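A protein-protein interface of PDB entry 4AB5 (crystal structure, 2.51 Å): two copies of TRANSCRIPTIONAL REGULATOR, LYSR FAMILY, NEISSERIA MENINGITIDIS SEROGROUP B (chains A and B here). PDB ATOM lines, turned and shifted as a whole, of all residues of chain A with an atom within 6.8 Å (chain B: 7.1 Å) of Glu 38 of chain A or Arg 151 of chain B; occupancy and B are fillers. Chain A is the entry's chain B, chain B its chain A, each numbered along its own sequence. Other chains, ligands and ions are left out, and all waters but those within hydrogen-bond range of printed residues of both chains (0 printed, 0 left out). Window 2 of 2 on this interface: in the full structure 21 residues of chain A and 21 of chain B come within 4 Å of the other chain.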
ATOM      1  N   ALA A   7     -32.201 -25.837  15.339  1.00  0.00           N
ATOM      2  CA  ALA A   7     -31.050 -24.937  15.288  1.00  0.00           C
ATOM      3  C   ALA A   7     -31.206 -23.822  14.232  1.00  0.00           C
ATOM      4  O   ALA A   7     -31.971 -23.964  13.280  1.00  0.00           O
ATOM      5  CB  ALA A   7     -29.784 -25.737  15.030  1.00  0.00           C
ATOM      6  N   GLY A   8     -30.480 -22.729  14.424  1.00  0.00           N
ATOM      7  CA  GLY A   8     -30.515 -21.576  13.532  1.00  0.00           C
ATOM      8  C   GLY A   8     -29.918 -20.313  14.128  1.00  0.00           C
ATOM      9  O   GLY A   8     -29.232 -20.358  15.153  1.00  0.00           O
ATOM     10  N   GLU A   9     -30.182 -19.172  13.477  1.00  0.00           N
ATOM     11  CA  GLU A   9     -29.673 -17.865  13.869  1.00  0.00           C
ATOM     12  C   GLU A   9     -30.749 -16.813  13.724  1.00  0.00           C
ATOM     13  O   GLU A   9     -31.388 -16.727  12.665  1.00  0.00           O
ATOM     14  CB  GLU A   9     -28.496 -17.460  12.965  1.00  0.00           C
ATOM     15  CG  GLU A   9     -27.117 -17.796  13.496  1.00  0.00           C
ATOM     16  CD  GLU A   9     -26.037 -17.748  12.433  1.00  0.00           C
ATOM     17  OE1 GLU A   9     -25.764 -16.645  11.903  1.00  0.00           O
ATOM     18  OE2 GLU A   9     -25.468 -18.819  12.122  1.00  0.00           O
ATOM     19  N   LEU A  10     -30.930 -15.991  14.780  1.00  0.00           N
ATOM     20  CA  LEU A  10     -31.856 -14.875  14.740  1.00  0.00           C
ATOM     21  C   LEU A  10     -31.110 -13.606  15.170  1.00  0.00           C
ATOM     22  O   LEU A  10     -31.047 -13.285  16.356  1.00  0.00           O
ATOM     23  CB  LEU A  10     -33.132 -15.151  15.559  1.00  0.00           C
ATOM     24  CG  LEU A  10     -34.206 -14.047  15.698  1.00  0.00           C
ATOM     25  CD1 LEU A  10     -34.499 -13.326  14.382  1.00  0.00           C
ATOM     26  CD2 LEU A  10     -35.481 -14.620  16.267  1.00  0.00           C
ATOM     27  N   ARG A  11     -30.481 -12.939  14.179  1.00  0.00           N
ATOM     28  CA  ARG A  11     -29.757 -11.681  14.350  1.00  0.00           C
ATOM     29  C   ARG A  11     -30.783 -10.588  14.040  1.00  0.00           C
ATOM     30  O   ARG A  11     -31.258 -10.479  12.902  1.00  0.00           O
ATOM     31  CB  ARG A  11     -28.523 -11.607  13.419  1.00  0.00           C
ATOM     32  CG  ARG A  11     -27.492 -12.722  13.656  1.00  0.00           C
ATOM     33  CD  ARG A  11     -26.496 -12.869  12.517  1.00  0.00           C
ATOM     34  NE  ARG A  11     -27.124 -13.322  11.270  1.00  0.00           N
ATOM     35  CZ  ARG A  11     -26.538 -13.300  10.078  1.00  0.00           C
ATOM     36  NH1 ARG A  11     -25.291 -12.873   9.951  1.00  0.00           N
ATOM     37  NH2 ARG A  11     -27.195 -13.706   9.001  1.00  0.00           N
ATOM     38  N   PHE A  30     -38.908 -15.873  23.699  1.00  0.00           N
ATOM     39  CA  PHE A  30     -38.472 -16.691  22.563  1.00  0.00           C
ATOM     40  C   PHE A  30     -37.331 -17.658  22.956  1.00  0.00           C
ATOM     41  O   PHE A  30     -37.381 -18.831  22.593  1.00  0.00           O
ATOM     42  CB  PHE A  30     -38.028 -15.774  21.403  1.00  0.00           C
ATOM     43  CG  PHE A  30     -37.445 -16.469  20.194  1.00  0.00           C
ATOM     44  CD1 PHE A  30     -36.078 -16.721  20.107  1.00  0.00           C
ATOM     45  CD2 PHE A  30     -38.252 -16.824  19.123  1.00  0.00           C
ATOM     46  CE1 PHE A  30     -35.537 -17.372  18.997  1.00  0.00           C
ATOM     47  CE2 PHE A  30     -37.707 -17.449  18.000  1.00  0.00           C
ATOM     48  CZ  PHE A  30     -36.357 -17.737  17.953  1.00  0.00           C
ATOM     49  N   TRP A  34     -36.940 -21.678  21.899  1.00  0.00           N
ATOM     50  CA  TRP A  34     -36.016 -22.001  20.810  1.00  0.00           C
ATOM     51  C   TRP A  34     -34.583 -21.927  21.348  1.00  0.00           C
ATOM     52  O   TRP A  34     -33.848 -21.026  20.959  1.00  0.00           O
ATOM     53  CB  TRP A  34     -36.214 -20.993  19.658  1.00  0.00           C
ATOM     54  CG  TRP A  34     -37.606 -20.989  19.101  1.00  0.00           C
ATOM     55  CD1 TRP A  34     -38.667 -20.252  19.541  1.00  0.00           C
ATOM     56  CD2 TRP A  34     -38.107 -21.829  18.055  1.00  0.00           C
ATOM     57  NE1 TRP A  34     -39.786 -20.543  18.798  1.00  0.00           N
ATOM     58  CE2 TRP A  34     -39.475 -21.520  17.886  1.00  0.00           C
ATOM     59  CE3 TRP A  34     -37.528 -22.810  17.234  1.00  0.00           C
ATOM     60  CZ2 TRP A  34     -40.266 -22.127  16.902  1.00  0.00           C
ATOM     61  CZ3 TRP A  34     -38.313 -23.416  16.264  1.00  0.00           C
ATOM     62  CH2 TRP A  34     -39.664 -23.074  16.105  1.00  0.00           C
ATOM     63  N   PRO A  35     -34.157 -22.815  22.282  1.00  0.00           N
ATOM     64  CA  PRO A  35     -32.800 -22.682  22.855  1.00  0.00           C
ATOM     65  C   PRO A  35     -31.621 -22.947  21.917  1.00  0.00           C
ATOM     66  O   PRO A  35     -30.486 -22.647  22.287  1.00  0.00           O
ATOM     67  CB  PRO A  35     -32.819 -23.673  24.022  1.00  0.00           C
ATOM     68  CG  PRO A  35     -33.793 -24.691  23.628  1.00  0.00           C
ATOM     69  CD  PRO A  35     -34.872 -23.951  22.898  1.00  0.00           C
ATOM     70  N   GLN A  36     -31.877 -23.516  20.724  1.00  0.00           N
ATOM     71  CA  GLN A  36     -30.839 -23.835  19.745  1.00  0.00           C
ATOM     72  C   GLN A  36     -30.602 -22.701  18.750  1.00  0.00           C
ATOM     73  O   GLN A  36     -29.601 -22.726  18.024  1.00  0.00           O
ATOM     74  CB  GLN A  36     -31.152 -25.160  19.026  1.00  0.00           C
ATOM     75  CG  GLN A  36     -31.170 -26.389  19.929  1.00  0.00           C
ATOM     76  CD  GLN A  36     -29.796 -26.714  20.445  1.00  0.00           C
ATOM     77  OE1 GLN A  36     -28.897 -27.104  19.695  1.00  0.00           O
ATOM     78  NE2 GLN A  36     -29.598 -26.544  21.741  1.00  0.00           N
ATOM     79  N   VAL A  37     -31.514 -21.710  18.720  1.00  0.00           N
ATOM     80  CA  VAL A  37     -31.461 -20.553  17.828  1.00  0.00           C
ATOM     81  C   VAL A  37     -30.593 -19.509  18.519  1.00  0.00           C
ATOM     82  O   VAL A  37     -30.934 -19.043  19.611  1.00  0.00           O
ATOM     83  CB  VAL A  37     -32.888 -20.023  17.464  1.00  0.00           C
ATOM     84  CG1 VAL A  37     -32.832 -18.697  16.706  1.00  0.00           C
ATOM     85  CG2 VAL A  37     -33.679 -21.056  16.672  1.00  0.00           C
ATOM     86  N   GLU A  38     -29.446 -19.183  17.906  1.00  0.00           N
ATOM     87  CA  GLU A  38     -28.513 -18.185  18.432  1.00  0.00           C
ATOM     88  C   GLU A  38     -29.062 -16.780  18.203  1.00  0.00           C
ATOM     89  O   GLU A  38     -29.314 -16.389  17.070  1.00  0.00           O
ATOM     90  CB  GLU A  38     -27.122 -18.351  17.804  1.00  0.00           C
ATOM     91  CG  GLU A  38     -26.368 -19.570  18.310  1.00  0.00           C
ATOM     92  CD  GLU A  38     -24.992 -19.758  17.703  1.00  0.00           C
ATOM     93  OE1 GLU A  38     -24.907 -20.114  16.504  1.00  0.00           O
ATOM     94  OE2 GLU A  38     -23.995 -19.577  18.440  1.00  0.00           O
ATOM     95  N   LEU A  39     -29.294 -16.047  19.289  1.00  0.00           N
ATOM     96  CA  LEU A  39     -29.843 -14.691  19.247  1.00  0.00           C
ATOM     97  C   LEU A  39     -28.748 -13.624  19.255  1.00  0.00           C
ATOM     98  O   LEU A  39     -27.702 -13.807  19.878  1.00  0.00           O
ATOM     99  CB  LEU A  39     -30.823 -14.468  20.417  1.00  0.00           C
ATOM    100  CG  LEU A  39     -32.215 -15.108  20.307  1.00  0.00           C
ATOM    101  CD1 LEU A  39     -32.893 -15.146  21.668  1.00  0.00           C
ATOM    102  CD2 LEU A  39     -33.109 -14.346  19.328  1.00  0.00           C
ATOM    103  N   ASP A  40     -28.999 -12.512  18.558  1.00  0.00           N
ATOM    104  CA  ASP A  40     -28.083 -11.376  18.467  1.00  0.00           C
ATOM    105  C   ASP A  40     -28.836 -10.104  18.108  1.00  0.00           C
ATOM    106  O   ASP A  40     -29.934 -10.179  17.550  1.00  0.00           O
ATOM    107  CB  ASP A  40     -26.958 -11.639  17.439  1.00  0.00           C
ATOM    108  CG  ASP A  40     -25.668 -10.873  17.697  1.00  0.00           C
ATOM    109  OD1 ASP A  40     -25.554 -10.238  18.767  1.00  0.00           O
ATOM    110  OD2 ASP A  40     -24.757 -10.946  16.853  1.00  0.00           O
ATOM    111  N   ILE A  41     -28.257  -8.935  18.459  1.00  0.00           N
ATOM    112  CA  ILE A  41     -28.804  -7.614  18.143  1.00  0.00           C
ATOM    113  C   ILE A  41     -27.781  -6.920  17.267  1.00  0.00           C
ATOM    114  O   ILE A  41     -26.628  -6.795  17.669  1.00  0.00           O
ATOM    115  CB  ILE A  41     -29.190  -6.771  19.399  1.00  0.00           C
ATOM    116  CG1 ILE A  41     -30.215  -7.517  20.298  1.00  0.00           C
ATOM    117  CG2 ILE A  41     -29.724  -5.377  18.980  1.00  0.00           C
ATOM    118  CD1 ILE A  41     -30.118  -7.225  21.756  1.00  0.00           C
ATOM    119  N   ASP A  59     -30.995 -11.461  10.151  1.00  0.00           N
ATOM    120  CA  ASP A  59     -32.050 -12.412   9.760  1.00  0.00           C
ATOM    121  C   ASP A  59     -33.475 -11.844   9.869  1.00  0.00           C
ATOM    122  O   ASP A  59     -34.369 -12.296   9.149  1.00  0.00           O
ATOM    123  CB  ASP A  59     -31.910 -13.727  10.540  1.00  0.00           C
ATOM    124  CG  ASP A  59     -30.494 -14.267  10.556  1.00  0.00           C
ATOM    125  OD1 ASP A  59     -30.078 -14.872   9.546  1.00  0.00           O
ATOM    126  OD2 ASP A  59     -29.791 -14.056  11.568  1.00  0.00           O
ATOM    127  N   ALA B  87     -24.518 -15.638  30.932  1.00  0.00           N
ATOM    128  CA  ALA B  87     -25.705 -16.455  30.723  1.00  0.00           C
ATOM    129  C   ALA B  87     -25.636 -17.666  31.673  1.00  0.00           C
ATOM    130  O   ALA B  87     -24.526 -18.083  32.015  1.00  0.00           O
ATOM    131  CB  ALA B  87     -25.760 -16.918  29.276  1.00  0.00           C
ATOM    132  N   HIS B  90     -23.103 -20.366  30.490  1.00  0.00           N
ATOM    133  CA  HIS B  90     -21.793 -19.834  30.111  1.00  0.00           C
ATOM    134  C   HIS B  90     -20.739 -20.523  30.992  1.00  0.00           C
ATOM    135  O   HIS B  90     -21.010 -20.721  32.181  1.00  0.00           O
ATOM    136  CB  HIS B  90     -21.761 -18.313  30.351  1.00  0.00           C
ATOM    137  CG  HIS B  90     -20.570 -17.632  29.760  1.00  0.00           C
ATOM    138  ND1 HIS B  90     -19.322 -17.715  30.355  1.00  0.00           N
ATOM    139  CD2 HIS B  90     -20.470 -16.881  28.639  1.00  0.00           C
ATOM    140  CE1 HIS B  90     -18.503 -17.045  29.567  1.00  0.00           C
ATOM    141  NE2 HIS B  90     -19.151 -16.516  28.527  1.00  0.00           N
ATOM    142  N   GLU B 106     -13.209 -13.702  26.602  1.00  0.00           N
ATOM    143  CA  GLU B 106     -14.574 -13.192  26.531  1.00  0.00           C
ATOM    144  C   GLU B 106     -14.754 -11.804  25.923  1.00  0.00           C
ATOM    145  O   GLU B 106     -13.916 -10.932  26.119  1.00  0.00           O
ATOM    146  CB  GLU B 106     -15.193 -13.231  27.945  1.00  0.00           C
ATOM    147  CG  GLU B 106     -15.816 -14.536  28.436  1.00  0.00           C
ATOM    148  CD  GLU B 106     -15.890 -15.778  27.572  1.00  0.00           C
ATOM    149  OE1 GLU B 106     -16.751 -15.797  26.665  1.00  0.00           O
ATOM    150  OE2 GLU B 106     -15.176 -16.765  27.861  1.00  0.00           O
ATOM    151  N   THR B 107     -15.892 -11.600  25.236  1.00  0.00           N
ATOM    152  CA  THR B 107     -16.330 -10.320  24.674  1.00  0.00           C
ATOM    153  C   THR B 107     -16.958  -9.547  25.846  1.00  0.00           C
ATOM    154  O   THR B 107     -17.807 -10.099  26.551  1.00  0.00           O
ATOM    155  CB  THR B 107     -17.336 -10.545  23.499  1.00  0.00           C
ATOM    156  OG1 THR B 107     -16.633 -11.054  22.373  1.00  0.00           O
ATOM    157  CG2 THR B 107     -18.065  -9.274  23.070  1.00  0.00           C
ATOM    158  N   LEU B 108     -16.533  -8.292  26.065  1.00  0.00           N
ATOM    159  CA  LEU B 108     -17.062  -7.453  27.142  1.00  0.00           C
ATOM    160  C   LEU B 108     -18.107  -6.472  26.609  1.00  0.00           C
ATOM    161  O   LEU B 108     -17.830  -5.706  25.690  1.00  0.00           O
ATOM    162  CB  LEU B 108     -15.916  -6.729  27.883  1.00  0.00           C
ATOM    163  CG  LEU B 108     -16.271  -5.976  29.196  1.00  0.00           C
ATOM    164  CD1 LEU B 108     -16.773  -6.922  30.296  1.00  0.00           C
ATOM    165  CD2 LEU B 108     -15.076  -5.178  29.695  1.00  0.00           C
ATOM    166  N   ILE B 109     -19.320  -6.530  27.161  1.00  0.00           N
ATOM    167  CA  ILE B 109     -20.416  -5.632  26.778  1.00  0.00           C
ATOM    168  C   ILE B 109     -20.492  -4.475  27.780  1.00  0.00           C
ATOM    169  O   ILE B 109     -20.600  -4.697  28.985  1.00  0.00           O
ATOM    170  CB  ILE B 109     -21.767  -6.364  26.527  1.00  0.00           C
ATOM    171  CG1 ILE B 109     -21.554  -7.624  25.655  1.00  0.00           C
ATOM    172  CG2 ILE B 109     -22.784  -5.406  25.861  1.00  0.00           C
ATOM    173  CD1 ILE B 109     -22.553  -8.661  25.817  1.00  0.00           C
ATOM    174  N   ARG B 135     -18.019  -4.886  22.877  1.00  0.00           N
ATOM    175  CA  ARG B 135     -19.338  -4.777  22.276  1.00  0.00           C
ATOM    176  C   ARG B 135     -19.995  -3.638  23.066  1.00  0.00           C
ATOM    177  O   ARG B 135     -19.769  -3.537  24.270  1.00  0.00           O
ATOM    178  CB  ARG B 135     -20.092  -6.102  22.467  1.00  0.00           C
ATOM    179  CG  ARG B 135     -21.393  -6.213  21.690  1.00  0.00           C
ATOM    180  CD  ARG B 135     -21.207  -6.826  20.311  1.00  0.00           C
ATOM    181  NE  ARG B 135     -22.436  -6.715  19.530  1.00  0.00           N
ATOM    182  CZ  ARG B 135     -23.255  -7.729  19.280  1.00  0.00           C
ATOM    183  NH1 ARG B 135     -22.970  -8.947  19.718  1.00  0.00           N
ATOM    184  NH2 ARG B 135     -24.356  -7.537  18.568  1.00  0.00           N
ATOM    185  N   GLN B 145     -29.841  -8.724  27.333  1.00  0.00           N
ATOM    186  CA  GLN B 145     -30.273  -9.666  26.291  1.00  0.00           C
ATOM    187  C   GLN B 145     -29.121 -10.236  25.490  1.00  0.00           C
ATOM    188  O   GLN B 145     -29.183 -11.397  25.085  1.00  0.00           O
ATOM    189  CB  GLN B 145     -31.362  -9.083  25.376  1.00  0.00           C
ATOM    190  CG  GLN B 145     -32.708  -8.849  26.077  1.00  0.00           C
ATOM    191  CD  GLN B 145     -33.279 -10.044  26.821  1.00  0.00           C
ATOM    192  OE1 GLN B 145     -33.243 -11.184  26.362  1.00  0.00           O
ATOM    193  NE2 GLN B 145     -33.866  -9.786  27.968  1.00  0.00           N
ATOM    194  N   LEU B 146     -28.066  -9.433  25.280  1.00  0.00           N
ATOM    195  CA  LEU B 146     -26.845  -9.830  24.587  1.00  0.00           C
ATOM    196  C   LEU B 146     -26.056 -10.809  25.459  1.00  0.00           C
ATOM    197  O   LEU B 146     -25.580 -11.826  24.956  1.00  0.00           O
ATOM    198  CB  LEU B 146     -25.998  -8.598  24.240  1.00  0.00           C
ATOM    199  CG  LEU B 146     -26.442  -7.763  23.036  1.00  0.00           C
ATOM    200  CD1 LEU B 146     -25.633  -6.488  22.937  1.00  0.00           C
ATOM    201  CD2 LEU B 146     -26.331  -8.552  21.740  1.00  0.00           C
ATOM    202  N   VAL B 147     -25.970 -10.529  26.776  1.00  0.00           N
ATOM    203  CA  VAL B 147     -25.305 -11.399  27.760  1.00  0.00           C
ATOM    204  C   VAL B 147     -26.040 -12.758  27.820  1.00  0.00           C
ATOM    205  O   VAL B 147     -25.395 -13.805  27.672  1.00  0.00           O
ATOM    206  CB  VAL B 147     -25.135 -10.716  29.159  1.00  0.00           C
ATOM    207  CG1 VAL B 147     -24.588 -11.689  30.192  1.00  0.00           C
ATOM    208  CG2 VAL B 147     -24.221  -9.490  29.069  1.00  0.00           C
ATOM    209  N   ALA B 148     -27.394 -12.724  27.955  1.00  0.00           N
ATOM    210  CA  ALA B 148     -28.275 -13.897  28.013  1.00  0.00           C
ATOM    211  C   ALA B 148     -28.193 -14.799  26.775  1.00  0.00           C
ATOM    212  O   ALA B 148     -28.388 -16.015  26.885  1.00  0.00           O
ATOM    213  CB  ALA B 148     -29.706 -13.450  28.233  1.00  0.00           C
ATOM    214  N   SER B 149     -27.888 -14.198  25.602  1.00  0.00           N
ATOM    215  CA  SER B 149     -27.774 -14.883  24.313  1.00  0.00           C
ATOM    216  C   SER B 149     -26.346 -15.377  24.072  1.00  0.00           C
ATOM    217  O   SER B 149     -26.038 -15.862  22.972  1.00  0.00           O
ATOM    218  CB  SER B 149     -28.232 -13.961  23.187  1.00  0.00           C
ATOM    219  OG  SER B 149     -29.551 -13.475  23.389  1.00  0.00           O
ATOM    220  N   ARG B 150     -25.485 -15.291  25.124  1.00  0.00           N
ATOM    221  CA  ARG B 150     -24.070 -15.697  25.127  1.00  0.00           C
ATOM    222  C   ARG B 150     -23.204 -14.890  24.146  1.00  0.00           C
ATOM    223  O   ARG B 150     -22.192 -15.390  23.657  1.00  0.00           O
ATOM    224  CB  ARG B 150     -23.906 -17.229  24.968  1.00  0.00           C
ATOM    225  CG  ARG B 150     -24.211 -17.988  26.254  1.00  0.00           C
ATOM    226  CD  ARG B 150     -23.913 -19.468  26.184  1.00  0.00           C
ATOM    227  NE  ARG B 150     -22.473 -19.720  26.135  1.00  0.00           N
ATOM    228  CZ  ARG B 150     -21.917 -20.924  26.174  1.00  0.00           C
ATOM    229  NH1 ARG B 150     -22.674 -22.010  26.289  1.00  0.00           N
ATOM    230  NH2 ARG B 150     -20.598 -21.054  26.104  1.00  0.00           N
ATOM    231  N   ARG B 151     -23.595 -13.623  23.890  1.00  0.00           N
ATOM    232  CA  ARG B 151     -22.891 -12.715  22.983  1.00  0.00           C
ATOM    233  C   ARG B 151     -21.773 -11.929  23.685  1.00  0.00           C
ATOM    234  O   ARG B 151     -21.120 -11.079  23.063  1.00  0.00           O
ATOM    235  CB  ARG B 151     -23.867 -11.788  22.216  1.00  0.00           C
ATOM    236  CG  ARG B 151     -24.949 -12.516  21.413  1.00  0.00           C
ATOM    237  CD  ARG B 151     -24.447 -13.097  20.106  1.00  0.00           C
ATOM    238  NE  ARG B 151     -23.736 -14.369  20.280  1.00  0.00           N
ATOM    239  CZ  ARG B 151     -24.300 -15.573  20.209  1.00  0.00           C
ATOM    240  NH1 ARG B 151     -25.603 -15.694  19.987  1.00  0.00           N
ATOM    241  NH2 ARG B 151     -23.562 -16.665  20.365  1.00  0.00           N
ATOM    242  N   GLY B 152     -21.541 -12.272  24.953  1.00  0.00           N
ATOM    243  CA  GLY B 152     -20.494 -11.706  25.786  1.00  0.00           C
ATOM    244  C   GLY B 152     -20.841 -11.716  27.257  1.00  0.00           C
ATOM    245  O   GLY B 152     -21.820 -12.349  27.670  1.00  0.00           O
ATOM    246  N   ILE B 153     -20.014 -11.023  28.059  1.00  0.00           N
ATOM    247  CA  ILE B 153     -20.197 -10.839  29.505  1.00  0.00           C
ATOM    248  C   ILE B 153     -20.205  -9.338  29.827  1.00  0.00           C
ATOM    249  O   ILE B 153     -19.816  -8.530  28.982  1.00  0.00           O
ATOM    250  CB  ILE B 153     -19.165 -11.635  30.361  1.00  0.00           C
ATOM    251  CG1 ILE B 153     -17.700 -11.222  30.050  1.00  0.00           C
ATOM    252  CG2 ILE B 153     -19.401 -13.153  30.246  1.00  0.00           C
ATOM    253  CD1 ILE B 153     -16.703 -11.687  31.082  1.00  0.00           C
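Of chain B, only Arg 151 comes within 4 Å of Glu 38 of chain A.
Arg 151 of chain B touches three residues of chain A.
Of the printed residues of chain B, Ile 41 of chain A touches Arg 135 (2.6 Å) and Leu 146 (3.8 Å).
Printed residues of chain A within 4 Å of Ser 149 of chain B: Leu 39.
Of the printed residues of chain B, Leu 39 of chain A touches Ser 149 and Arg 151.
The nearest printed residue of chain B that does not touch Asp 40 of chain A is Ser 149 of chain B (4.9 Å).
Among the printed residues, pairs that only touch across the chains: Asp 40 of chain A with Arg 151 of chain B (3.3 Å), Leu 39 of chain A with Ser 149 of chain B (3.4 Å), Asp 40 of chain A with Leu 146 of chain B (3.5 Å) and Ile 41 of chain A with Leu 146 of chain B (3.8 Å).
No position is printed for both chains.
Of the 8 pairs that touch across the chains among the printed residues, none has its exchanged pair printed and touching as well.
The guanidinium group (NH2) of Arg 135 of chain B is in salt-bridge range of the side-chain carboxylate (OD1) of Asp 40 of chain A (3.0 Å).
The guanidinium group (NH2) of Arg 135 of chain B lies within hydrogen-bond range of the backbone carbonyl oxygen (O) of Ile 41 of chain A.
NH1 of Arg 151 of chain B is in hydrogen-bond range of O of Leu 39 of chain A, at 2.8 Å.
The guanidinium group (NH2) of Arg 151 of chain B is in salt-bridge range of the side-chain carboxylate (OE2) of Glu 38 of chain A (3.5 Å).
The backbone NH (N) of Glu 38 of chain A sits at hydrogen-bond distance from the backbone carbonyl oxygen (O) of Gly 8 of chain A, at 3.0 Å.
The backbone carbonyl oxygen of Leu 10 of chain A sits at hydrogen-bond distance from the backbone NH of Asp 40 of chain A (3.1 Å).
The backbone NH of Arg 151 of chain B sits at hydrogen-bond distance from the backbone carbonyl oxygen of Leu 146 of chain B (2.9 Å).
The backbone carbonyl oxygen (O) of Ser 149 of chain B is in hydrogen-bond range of the guanidinium group (NH1) of Arg 151 of chain B (3.0 Å).
N of Arg 135 of chain B sits at hydrogen-bond distance from O of Leu 108 of chain B, at 2.9 Å.
The backbone NH (N) of Leu 10 of chain A is in hydrogen-bond range of the backbone carbonyl oxygen (O) of Glu 38 of chain A, 2.8 Å away.
Hydrophobic or aromatic side chains of chain A that line the printed part of chain B: Leu 39 and Ile 41.
Among the printed residues, 8 pairs touch across the chains.
Among the printed residues, Asp or Glu carboxylates within 4 Å of a Lys or Arg side-chain nitrogen of the other chain: Glu 38 of chain A with Arg 151 of chain B (3.5 Å) and Asp 40 of chain A with Arg 135 of chain B (3.0 Å).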
